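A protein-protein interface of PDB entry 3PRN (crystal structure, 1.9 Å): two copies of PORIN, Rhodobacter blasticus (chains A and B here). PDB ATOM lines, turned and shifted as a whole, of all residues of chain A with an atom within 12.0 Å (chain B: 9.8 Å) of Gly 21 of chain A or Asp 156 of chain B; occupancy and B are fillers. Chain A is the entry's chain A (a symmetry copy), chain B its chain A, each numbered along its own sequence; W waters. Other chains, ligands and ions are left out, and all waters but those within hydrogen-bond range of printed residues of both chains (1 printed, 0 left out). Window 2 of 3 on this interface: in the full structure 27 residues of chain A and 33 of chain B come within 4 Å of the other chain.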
ATOM      1  N   TYR A  14      22.096  -8.015 -19.534  1.00  0.00           N
ATOM      2  CA  TYR A  14      23.334  -8.673 -19.982  1.00  0.00           C
ATOM      3  C   TYR A  14      23.010  -9.732 -21.029  1.00  0.00           C
ATOM      4  O   TYR A  14      22.115 -10.561 -20.863  1.00  0.00           O
ATOM      5  CB  TYR A  14      24.052  -9.286 -18.782  1.00  0.00           C
ATOM      6  CG  TYR A  14      25.179 -10.246 -19.134  1.00  0.00           C
ATOM      7  CD1 TYR A  14      26.456  -9.787 -19.400  1.00  0.00           C
ATOM      8  CD2 TYR A  14      24.929 -11.612 -19.218  1.00  0.00           C
ATOM      9  CE1 TYR A  14      27.487 -10.668 -19.710  1.00  0.00           C
ATOM     10  CE2 TYR A  14      25.940 -12.513 -19.525  1.00  0.00           C
ATOM     11  CZ  TYR A  14      27.223 -12.029 -19.750  1.00  0.00           C
ATOM     12  OH  TYR A  14      28.222 -12.928 -20.081  1.00  0.00           O
ATOM     13  N   VAL A  15      23.777  -9.662 -22.112  1.00  0.00           N
ATOM     14  CA  VAL A  15      23.669 -10.587 -23.224  1.00  0.00           C
ATOM     15  C   VAL A  15      25.107 -11.089 -23.518  1.00  0.00           C
ATOM     16  O   VAL A  15      25.935 -10.255 -23.897  1.00  0.00           O
ATOM     17  CB  VAL A  15      23.144  -9.960 -24.513  1.00  0.00           C
ATOM     18  CG1 VAL A  15      23.260 -11.042 -25.602  1.00  0.00           C
ATOM     19  CG2 VAL A  15      21.703  -9.511 -24.324  1.00  0.00           C
ATOM     20  N   GLU A  16      25.346 -12.340 -23.171  1.00  0.00           N
ATOM     21  CA  GLU A  16      26.701 -12.888 -23.342  1.00  0.00           C
ATOM     22  C   GLU A  16      27.174 -12.715 -24.789  1.00  0.00           C
ATOM     23  O   GLU A  16      26.411 -13.012 -25.711  1.00  0.00           O
ATOM     24  CB  GLU A  16      26.737 -14.350 -22.955  1.00  0.00           C
ATOM     25  CG  GLU A  16      28.184 -14.881 -22.993  1.00  0.00           C
ATOM     26  CD  GLU A  16      28.240 -16.297 -22.422  1.00  0.00           C
ATOM     27  OE1 GLU A  16      27.281 -17.086 -22.699  1.00  0.00           O
ATOM     28  OE2 GLU A  16      29.233 -16.593 -21.723  1.00  0.00           O
ATOM     29  N   ASP A  17      28.383 -12.163 -24.942  1.00  0.00           N
ATOM     30  CA  ASP A  17      28.978 -11.911 -26.248  1.00  0.00           C
ATOM     31  C   ASP A  17      28.015 -11.303 -27.246  1.00  0.00           C
ATOM     32  O   ASP A  17      27.762 -11.831 -28.338  1.00  0.00           O
ATOM     33  CB  ASP A  17      29.621 -13.166 -26.840  1.00  0.00           C
ATOM     34  CG  ASP A  17      30.687 -13.784 -25.966  1.00  0.00           C
ATOM     35  OD1 ASP A  17      31.464 -13.100 -25.234  1.00  0.00           O
ATOM     36  OD2 ASP A  17      30.756 -15.058 -25.991  1.00  0.00           O
ATOM     37  N   ARG A  18      27.486 -10.126 -26.896  1.00  0.00           N
ATOM     38  CA  ARG A  18      26.520  -9.408 -27.706  1.00  0.00           C
ATOM     39  C   ARG A  18      26.978  -9.061 -29.104  1.00  0.00           C
ATOM     40  O   ARG A  18      26.152  -8.945 -30.028  1.00  0.00           O
ATOM     41  CB  ARG A  18      26.201  -8.110 -26.941  1.00  0.00           C
ATOM     42  CG  ARG A  18      24.856  -7.506 -27.217  1.00  0.00           C
ATOM     43  CD  ARG A  18      24.767  -6.154 -26.529  1.00  0.00           C
ATOM     44  NE  ARG A  18      24.304  -6.240 -25.147  1.00  0.00           N
ATOM     45  CZ  ARG A  18      23.032  -6.189 -24.737  1.00  0.00           C
ATOM     46  NH1 ARG A  18      22.035  -6.103 -25.605  1.00  0.00           N
ATOM     47  NH2 ARG A  18      22.750  -6.237 -23.434  1.00  0.00           N
ATOM     48  N   GLY A  19      28.275  -8.822 -29.329  1.00  0.00           N
ATOM     49  CA  GLY A  19      28.660  -8.426 -30.718  1.00  0.00           C
ATOM     50  C   GLY A  19      30.045  -7.806 -30.641  1.00  0.00           C
ATOM     51  O   GLY A  19      30.460  -7.306 -29.573  1.00  0.00           O
ATOM     52  N   VAL A  20      30.771  -7.852 -31.756  1.00  0.00           N
ATOM     53  CA  VAL A  20      32.138  -7.299 -31.774  1.00  0.00           C
ATOM     54  C   VAL A  20      32.148  -5.808 -31.448  1.00  0.00           C
ATOM     55  O   VAL A  20      31.442  -5.046 -32.104  1.00  0.00           O
ATOM     56  CB  VAL A  20      32.794  -7.549 -33.151  1.00  0.00           C
ATOM     57  CG1 VAL A  20      33.339  -8.978 -33.239  1.00  0.00           C
ATOM     58  CG2 VAL A  20      31.773  -7.330 -34.279  1.00  0.00           C
ATOM     59  N   GLY A  21      32.925  -5.383 -30.453  1.00  0.00           N
ATOM     60  CA  GLY A  21      32.990  -3.975 -30.086  1.00  0.00           C
ATOM     61  C   GLY A  21      31.786  -3.444 -29.308  1.00  0.00           C
ATOM     62  O   GLY A  21      31.671  -2.226 -29.133  1.00  0.00           O
ATOM     63  N   LEU A  22      30.904  -4.321 -28.849  1.00  0.00           N
ATOM     64  CA  LEU A  22      29.731  -3.926 -28.075  1.00  0.00           C
ATOM     65  C   LEU A  22      29.891  -4.296 -26.617  1.00  0.00           C
ATOM     66  O   LEU A  22      30.465  -5.327 -26.289  1.00  0.00           O
ATOM     67  CB  LEU A  22      28.445  -4.558 -28.626  1.00  0.00           C
ATOM     68  CG  LEU A  22      28.113  -4.230 -30.083  1.00  0.00           C
ATOM     69  CD1 LEU A  22      26.841  -4.949 -30.507  1.00  0.00           C
ATOM     70  CD2 LEU A  22      27.970  -2.731 -30.302  1.00  0.00           C
ATOM     71  N   GLU A  23      29.333  -3.510 -25.716  1.00  0.00           N
ATOM     72  CA  GLU A  23      29.283  -3.843 -24.305  1.00  0.00           C
ATOM     73  C   GLU A  23      28.266  -4.973 -24.118  1.00  0.00           C
ATOM     74  O   GLU A  23      27.160  -4.872 -24.633  1.00  0.00           O
ATOM     75  CB  GLU A  23      28.730  -2.665 -23.477  1.00  0.00           C
ATOM     76  CG  GLU A  23      29.715  -1.596 -23.106  1.00  0.00           C
ATOM     77  CD  GLU A  23      30.952  -2.111 -22.383  1.00  0.00           C
ATOM     78  OE1 GLU A  23      30.877  -3.183 -21.745  1.00  0.00           O
ATOM     79  OE2 GLU A  23      32.002  -1.433 -22.467  1.00  0.00           O
ATOM     80  N   ASP A  24      28.557  -5.992 -23.355  1.00  0.00           N
ATOM     81  CA  ASP A  24      27.601  -7.049 -23.136  1.00  0.00           C
ATOM     82  C   ASP A  24      26.486  -6.595 -22.164  1.00  0.00           C
ATOM     83  O   ASP A  24      25.370  -7.059 -22.294  1.00  0.00           O
ATOM     84  CB  ASP A  24      28.317  -8.208 -22.383  1.00  0.00           C
ATOM     85  CG  ASP A  24      29.029  -9.137 -23.382  1.00  0.00           C
ATOM     86  OD1 ASP A  24      28.829  -9.029 -24.598  1.00  0.00           O
ATOM     87  OD2 ASP A  24      29.736 -10.015 -22.837  1.00  0.00           O
ATOM     88  N   THR A  25      26.897  -5.741 -21.237  1.00  0.00           N
ATOM     89  CA  THR A  25      25.937  -5.256 -20.247  1.00  0.00           C
ATOM     90  C   THR A  25      25.527  -3.817 -20.516  1.00  0.00           C
ATOM     91  O   THR A  25      26.405  -2.935 -20.692  1.00  0.00           O
ATOM     92  CB  THR A  25      26.563  -5.378 -18.838  1.00  0.00           C
ATOM     93  OG1 THR A  25      26.689  -6.768 -18.459  1.00  0.00           O
ATOM     94  CG2 THR A  25      25.638  -4.769 -17.766  1.00  0.00           C
ATOM     95  N   ILE A  26      24.229  -3.541 -20.666  1.00  0.00           N
ATOM     96  CA  ILE A  26      23.823  -2.139 -20.818  1.00  0.00           C
ATOM     97  C   ILE A  26      22.740  -1.767 -19.761  1.00  0.00           C
ATOM     98  O   ILE A  26      22.207  -2.655 -19.111  1.00  0.00           O
ATOM     99  CB  ILE A  26      23.219  -1.830 -22.201  1.00  0.00           C
ATOM    100  CG1 ILE A  26      21.946  -2.645 -22.403  1.00  0.00           C
ATOM    101  CG2 ILE A  26      24.256  -2.020 -23.291  1.00  0.00           C
ATOM    102  CD1 ILE A  26      21.185  -2.289 -23.653  1.00  0.00           C
ATOM    103  N   ILE A  27      22.454  -0.480 -19.624  1.00  0.00           N
ATOM    104  CA  ILE A  27      21.319  -0.052 -18.775  1.00  0.00           C
ATOM    105  C   ILE A  27      20.094   0.031 -19.651  1.00  0.00           C
ATOM    106  O   ILE A  27      20.041   0.875 -20.587  1.00  0.00           O
ATOM    107  CB  ILE A  27      21.548   1.285 -18.081  1.00  0.00           C
ATOM    108  CG1 ILE A  27      22.625   0.995 -16.985  1.00  0.00           C
ATOM    109  CG2 ILE A  27      20.310   1.869 -17.414  1.00  0.00           C
ATOM    110  CD1 ILE A  27      23.296   2.277 -16.544  1.00  0.00           C
ATOM    111  N   TYR B 148      27.687  11.357 -14.631  1.00  0.00           N
ATOM    112  CA  TYR B 148      28.519  10.577 -15.560  1.00  0.00           C
ATOM    113  C   TYR B 148      27.694  10.324 -16.816  1.00  0.00           C
ATOM    114  O   TYR B 148      26.546   9.806 -16.705  1.00  0.00           O
ATOM    115  CB  TYR B 148      28.907   9.265 -14.852  1.00  0.00           C
ATOM    116  CG  TYR B 148      29.433   8.224 -15.812  1.00  0.00           C
ATOM    117  CD1 TYR B 148      30.752   8.250 -16.261  1.00  0.00           C
ATOM    118  CD2 TYR B 148      28.572   7.241 -16.271  1.00  0.00           C
ATOM    119  CE1 TYR B 148      31.201   7.274 -17.163  1.00  0.00           C
ATOM    120  CE2 TYR B 148      28.998   6.258 -17.158  1.00  0.00           C
ATOM    121  CZ  TYR B 148      30.317   6.311 -17.604  1.00  0.00           C
ATOM    122  OH  TYR B 148      30.717   5.327 -18.501  1.00  0.00           O
ATOM    123  N   ASP B 150      27.568   8.712 -20.686  1.00  0.00           N
ATOM    124  CA  ASP B 150      28.211   7.936 -21.775  1.00  0.00           C
ATOM    125  C   ASP B 150      27.373   8.239 -23.001  1.00  0.00           C
ATOM    126  O   ASP B 150      26.183   7.877 -23.048  1.00  0.00           O
ATOM    127  CB  ASP B 150      28.138   6.485 -21.352  1.00  0.00           C
ATOM    128  CG  ASP B 150      28.779   5.538 -22.366  1.00  0.00           C
ATOM    129  OD1 ASP B 150      28.985   5.938 -23.503  1.00  0.00           O
ATOM    130  OD2 ASP B 150      28.987   4.363 -21.990  1.00  0.00           O
ATOM    131  N   PRO B 151      27.904   8.879 -24.015  1.00  0.00           N
ATOM    132  CA  PRO B 151      27.129   9.230 -25.202  1.00  0.00           C
ATOM    133  C   PRO B 151      26.734   8.089 -26.069  1.00  0.00           C
ATOM    134  O   PRO B 151      25.848   8.199 -26.963  1.00  0.00           O
ATOM    135  CB  PRO B 151      28.011  10.229 -25.911  1.00  0.00           C
ATOM    136  CG  PRO B 151      29.397  10.051 -25.381  1.00  0.00           C
ATOM    137  CD  PRO B 151      29.300   9.373 -24.045  1.00  0.00           C
ATOM    138  N   ASP B 152      27.335   6.906 -25.901  1.00  0.00           N
ATOM    139  CA  ASP B 152      26.893   5.757 -26.673  1.00  0.00           C
ATOM    140  C   ASP B 152      27.191   4.526 -25.821  1.00  0.00           C
ATOM    141  O   ASP B 152      28.258   3.876 -25.968  1.00  0.00           O
ATOM    142  CB  ASP B 152      27.556   5.620 -28.053  1.00  0.00           C
ATOM    143  CG  ASP B 152      26.908   4.506 -28.868  1.00  0.00           C
ATOM    144  OD1 ASP B 152      26.326   3.514 -28.363  1.00  0.00           O
ATOM    145  OD2 ASP B 152      27.003   4.591 -30.109  1.00  0.00           O
ATOM    146  N   GLN B 153      26.237   4.190 -24.962  1.00  0.00           N
ATOM    147  CA  GLN B 153      26.400   3.100 -24.024  1.00  0.00           C
ATOM    148  C   GLN B 153      26.461   1.714 -24.624  1.00  0.00           C
ATOM    149  O   GLN B 153      26.814   0.764 -23.893  1.00  0.00           O
ATOM    150  CB  GLN B 153      25.281   3.157 -22.941  1.00  0.00           C
ATOM    151  CG  GLN B 153      23.946   2.581 -23.479  1.00  0.00           C
ATOM    152  CD  GLN B 153      23.035   2.166 -22.313  1.00  0.00           C
ATOM    153  OE1 GLN B 153      23.520   1.841 -21.221  1.00  0.00           O
ATOM    154  NE2 GLN B 153      21.729   2.154 -22.552  1.00  0.00           N
ATOM    155  N   THR B 154      26.101   1.476 -25.852  1.00  0.00           N
ATOM    156  CA  THR B 154      26.108   0.122 -26.372  1.00  0.00           C
ATOM    157  C   THR B 154      27.520  -0.229 -26.883  1.00  0.00           C
ATOM    158  O   THR B 154      27.848  -1.413 -26.958  1.00  0.00           O
ATOM    159  CB  THR B 154      25.133  -0.046 -27.560  1.00  0.00           C
ATOM    160  OG1 THR B 154      25.584   0.883 -28.544  1.00  0.00           O
ATOM    161  CG2 THR B 154      23.699   0.310 -27.189  1.00  0.00           C
ATOM    162  N   VAL B 155      28.315   0.746 -27.210  1.00  0.00           N
ATOM    163  CA  VAL B 155      29.656   0.469 -27.798  1.00  0.00           C
ATOM    164  C   VAL B 155      30.670   0.298 -26.703  1.00  0.00           C
ATOM    165  O   VAL B 155      30.550   0.918 -25.613  1.00  0.00           O
ATOM    166  CB  VAL B 155      30.012   1.677 -28.693  1.00  0.00           C
ATOM    167  CG1 VAL B 155      31.501   1.768 -28.908  1.00  0.00           C
ATOM    168  CG2 VAL B 155      29.224   1.591 -29.994  1.00  0.00           C
ATOM    169  N   ASP B 156      31.678  -0.542 -26.887  1.00  0.00           N
ATOM    170  CA  ASP B 156      32.687  -0.737 -25.867  1.00  0.00           C
ATOM    171  C   ASP B 156      33.154   0.564 -25.214  1.00  0.00           C
ATOM    172  O   ASP B 156      33.538   1.549 -25.853  1.00  0.00           O
ATOM    173  CB  ASP B 156      33.952  -1.358 -26.535  1.00  0.00           C
ATOM    174  CG  ASP B 156      34.705  -2.061 -25.417  1.00  0.00           C
ATOM    175  OD1 ASP B 156      35.542  -1.396 -24.699  1.00  0.00           O
ATOM    176  OD2 ASP B 156      34.445  -3.293 -25.157  1.00  0.00           O
ATOM    177  N   SER B 157      33.199   0.559 -23.915  1.00  0.00           N
ATOM    178  CA  SER B 157      33.541   1.678 -23.072  1.00  0.00           C
ATOM    179  C   SER B 157      34.836   2.401 -23.374  1.00  0.00           C
ATOM    180  O   SER B 157      34.962   3.631 -23.210  1.00  0.00           O
ATOM    181  CB  SER B 157      33.609   1.094 -21.637  1.00  0.00           C
ATOM    182  OG  SER B 157      33.426   2.133 -20.717  1.00  0.00           O
ATOM    183  N   SER B 158      35.874   1.681 -23.821  1.00  0.00           N
ATOM    184  CA  SER B 158      37.148   2.364 -24.132  1.00  0.00           C
ATOM    185  C   SER B 158      37.128   2.979 -25.511  1.00  0.00           C
ATOM    186  O   SER B 158      38.072   3.694 -25.929  1.00  0.00           O
ATOM    187  CB  SER B 158      38.267   1.305 -24.018  1.00  0.00           C
ATOM    188  OG  SER B 158      37.987   0.337 -25.052  1.00  0.00           O
ATOM    189  N   LEU B 159      36.079   2.770 -26.297  1.00  0.00           N
ATOM    190  CA  LEU B 159      36.018   3.376 -27.620  1.00  0.00           C
ATOM    191  C   LEU B 159      35.278   4.703 -27.653  1.00  0.00           C
ATOM    192  O   LEU B 159      35.113   5.298 -28.746  1.00  0.00           O
ATOM    193  CB  LEU B 159      35.349   2.362 -28.576  1.00  0.00           C
ATOM    194  CG  LEU B 159      36.162   1.041 -28.707  1.00  0.00           C
ATOM    195  CD1 LEU B 159      35.365  -0.039 -29.390  1.00  0.00           C
ATOM    196  CD2 LEU B 159      37.441   1.328 -29.492  1.00  0.00           C
ATOM    197  N   VAL B 160      34.717   5.175 -26.527  1.00  0.00           N
ATOM    198  CA  VAL B 160      33.955   6.447 -26.554  1.00  0.00           C
ATOM    199  C   VAL B 160      34.443   7.350 -25.443  1.00  0.00           C
ATOM    200  O   VAL B 160      35.031   6.887 -24.462  1.00  0.00           O
ATOM    201  CB  VAL B 160      32.427   6.214 -26.453  1.00  0.00           C
ATOM    202  CG1 VAL B 160      31.966   5.379 -27.655  1.00  0.00           C
ATOM    203  CG2 VAL B 160      32.018   5.496 -25.206  1.00  0.00           C
ATOM    204  N   THR B 161      34.240   8.631 -25.534  1.00  0.00           N
ATOM    205  CA  THR B 161      34.680   9.522 -24.460  1.00  0.00           C
ATOM    206  C   THR B 161      33.502   9.797 -23.535  1.00  0.00           C
ATOM    207  O   THR B 161      32.507  10.331 -24.012  1.00  0.00           O
ATOM    208  CB  THR B 161      35.113  10.876 -25.082  1.00  0.00           C
ATOM    209  OG1 THR B 161      36.069  10.590 -26.109  1.00  0.00           O
ATOM    210  CG2 THR B 161      35.641  11.844 -24.066  1.00  0.00           C
ATOM    211  N   GLU B 162      33.610   9.479 -22.282  1.00  0.00           N
ATOM    212  CA  GLU B 162      32.507   9.735 -21.348  1.00  0.00           C
ATOM    213  C   GLU B 162      32.777  11.032 -20.599  1.00  0.00           C
ATOM    214  O   GLU B 162      33.939  11.380 -20.428  1.00  0.00           O
ATOM    215  CB  GLU B 162      32.380   8.571 -20.348  1.00  0.00           C
ATOM    216  CG  GLU B 162      31.914   7.306 -21.074  1.00  0.00           C
ATOM    217  CD  GLU B 162      33.073   6.416 -21.468  1.00  0.00           C
ATOM    218  OE1 GLU B 162      34.186   6.531 -20.911  1.00  0.00           O
ATOM    219  OE2 GLU B 162      32.900   5.566 -22.379  1.00  0.00           O
HETATM  220  O   HOH W   1      25.855  -3.193 -26.418  1.00  0.00           O
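Among the printed residues, merely in contact across the chains: Gly 21 of chain A with Val 155 of chain B (3.6 Å), Leu 22 of chain A with Thr 154 of chain B (3.3 Å), Glu 23 of chain A with Gln 153 of chain B (3.8 Å), Glu 23 of chain A with Val 155 of chain B (3.6 Å), Glu 23 of chain A with Asp 156 of chain B (3.5 Å) and Ile 26 of chain A with Gln 153 of chain B (3.8 Å).
The backbone carbonyl oxygen of Ile 27 of chain A is in hydrogen-bond range of the side-chain amide nitrogen of Gln 153 of chain B (2.9 Å). N of Glu 23 of chain A sits at hydrogen-bond distance from O of Thr 154 of chain B, 2.9 Å away. The backbone NH (N) of Asp 156 of chain B is in hydrogen-bond range of the backbone carbonyl oxygen (O) of Gly 21 of chain A, at 2.8 Å. N of Ser 157 of chain B sits at hydrogen-bond distance from OE2 of Glu 23 of chain A.
Water W1 bridges O of Thr 154 of chain B and O of Glu 23 of chain A.
No position is printed for both chains.
Of the 14 printed residues of chain A, 5 touch a printed residue of chain B. Printed residues of chain A that touch a printed residue of chain B: Gly 21, Leu 22, Glu 23, Ile 26 and Ile 27. Hydrophobic or aromatic side chains of chain A within 4 Å of the printed part of chain B: Leu 22, Ile 26 and Ile 27. Among the printed residues, 10 pairs touch across the chains. Among the printed residues, no Asp or Glu carboxylate lies within 4 Å of a Lys or Arg side-chain nitrogen of the other chain.
Of the printed residues of chain B, Gly 21 of chain A touches Val 155 and Asp 156. Leu 22 of chain A touches just one residue of chain B: Thr 154 (3.3 Å). Printed residues of chain B within 4 Å of Ile 27 of chain A: Gln 153. Printed residues of chain A within 4 Å of Gln 153 of chain B: Glu 23, Ile 26 and Ile 27. Val 155 of chain B touches just these residues of chain A: Gly 21 (3.6 Å) and Glu 23 (3.6 Å). Asp 156 of chain B touches two residues of chain A. Ser 157 of chain B touches just one residue of chain A: Glu 23 (2.7 Å). No residue of chain A comes within 4 Å of Ser 158 of chain B. No residue of chain A comes within 4 Å of Leu 159 of chain B. The nearest residue of chain B that does not touch Gly 21 of chain A is Leu 159 of chain B (4.3 Å). The nearest printed residue of chain B that does not touch Ile 27 of chain A is Tyr 148 of chain B (7.0 Å).
OD1 of Asp 152 of chain B lies within hydrogen-bond range of OG1 of Thr 154 of chain B, at 2.7 Å. OD1 of Asp 156 of chain B lies within hydrogen-bond range of OG of Ser 158 of chain B (3.0 Å). The guanidinium group (NE) of Arg 18 of chain A lies within hydrogen-bond range of the backbone carbonyl oxygen (O) of Glu 23 of chain A, 3.2 Å away.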
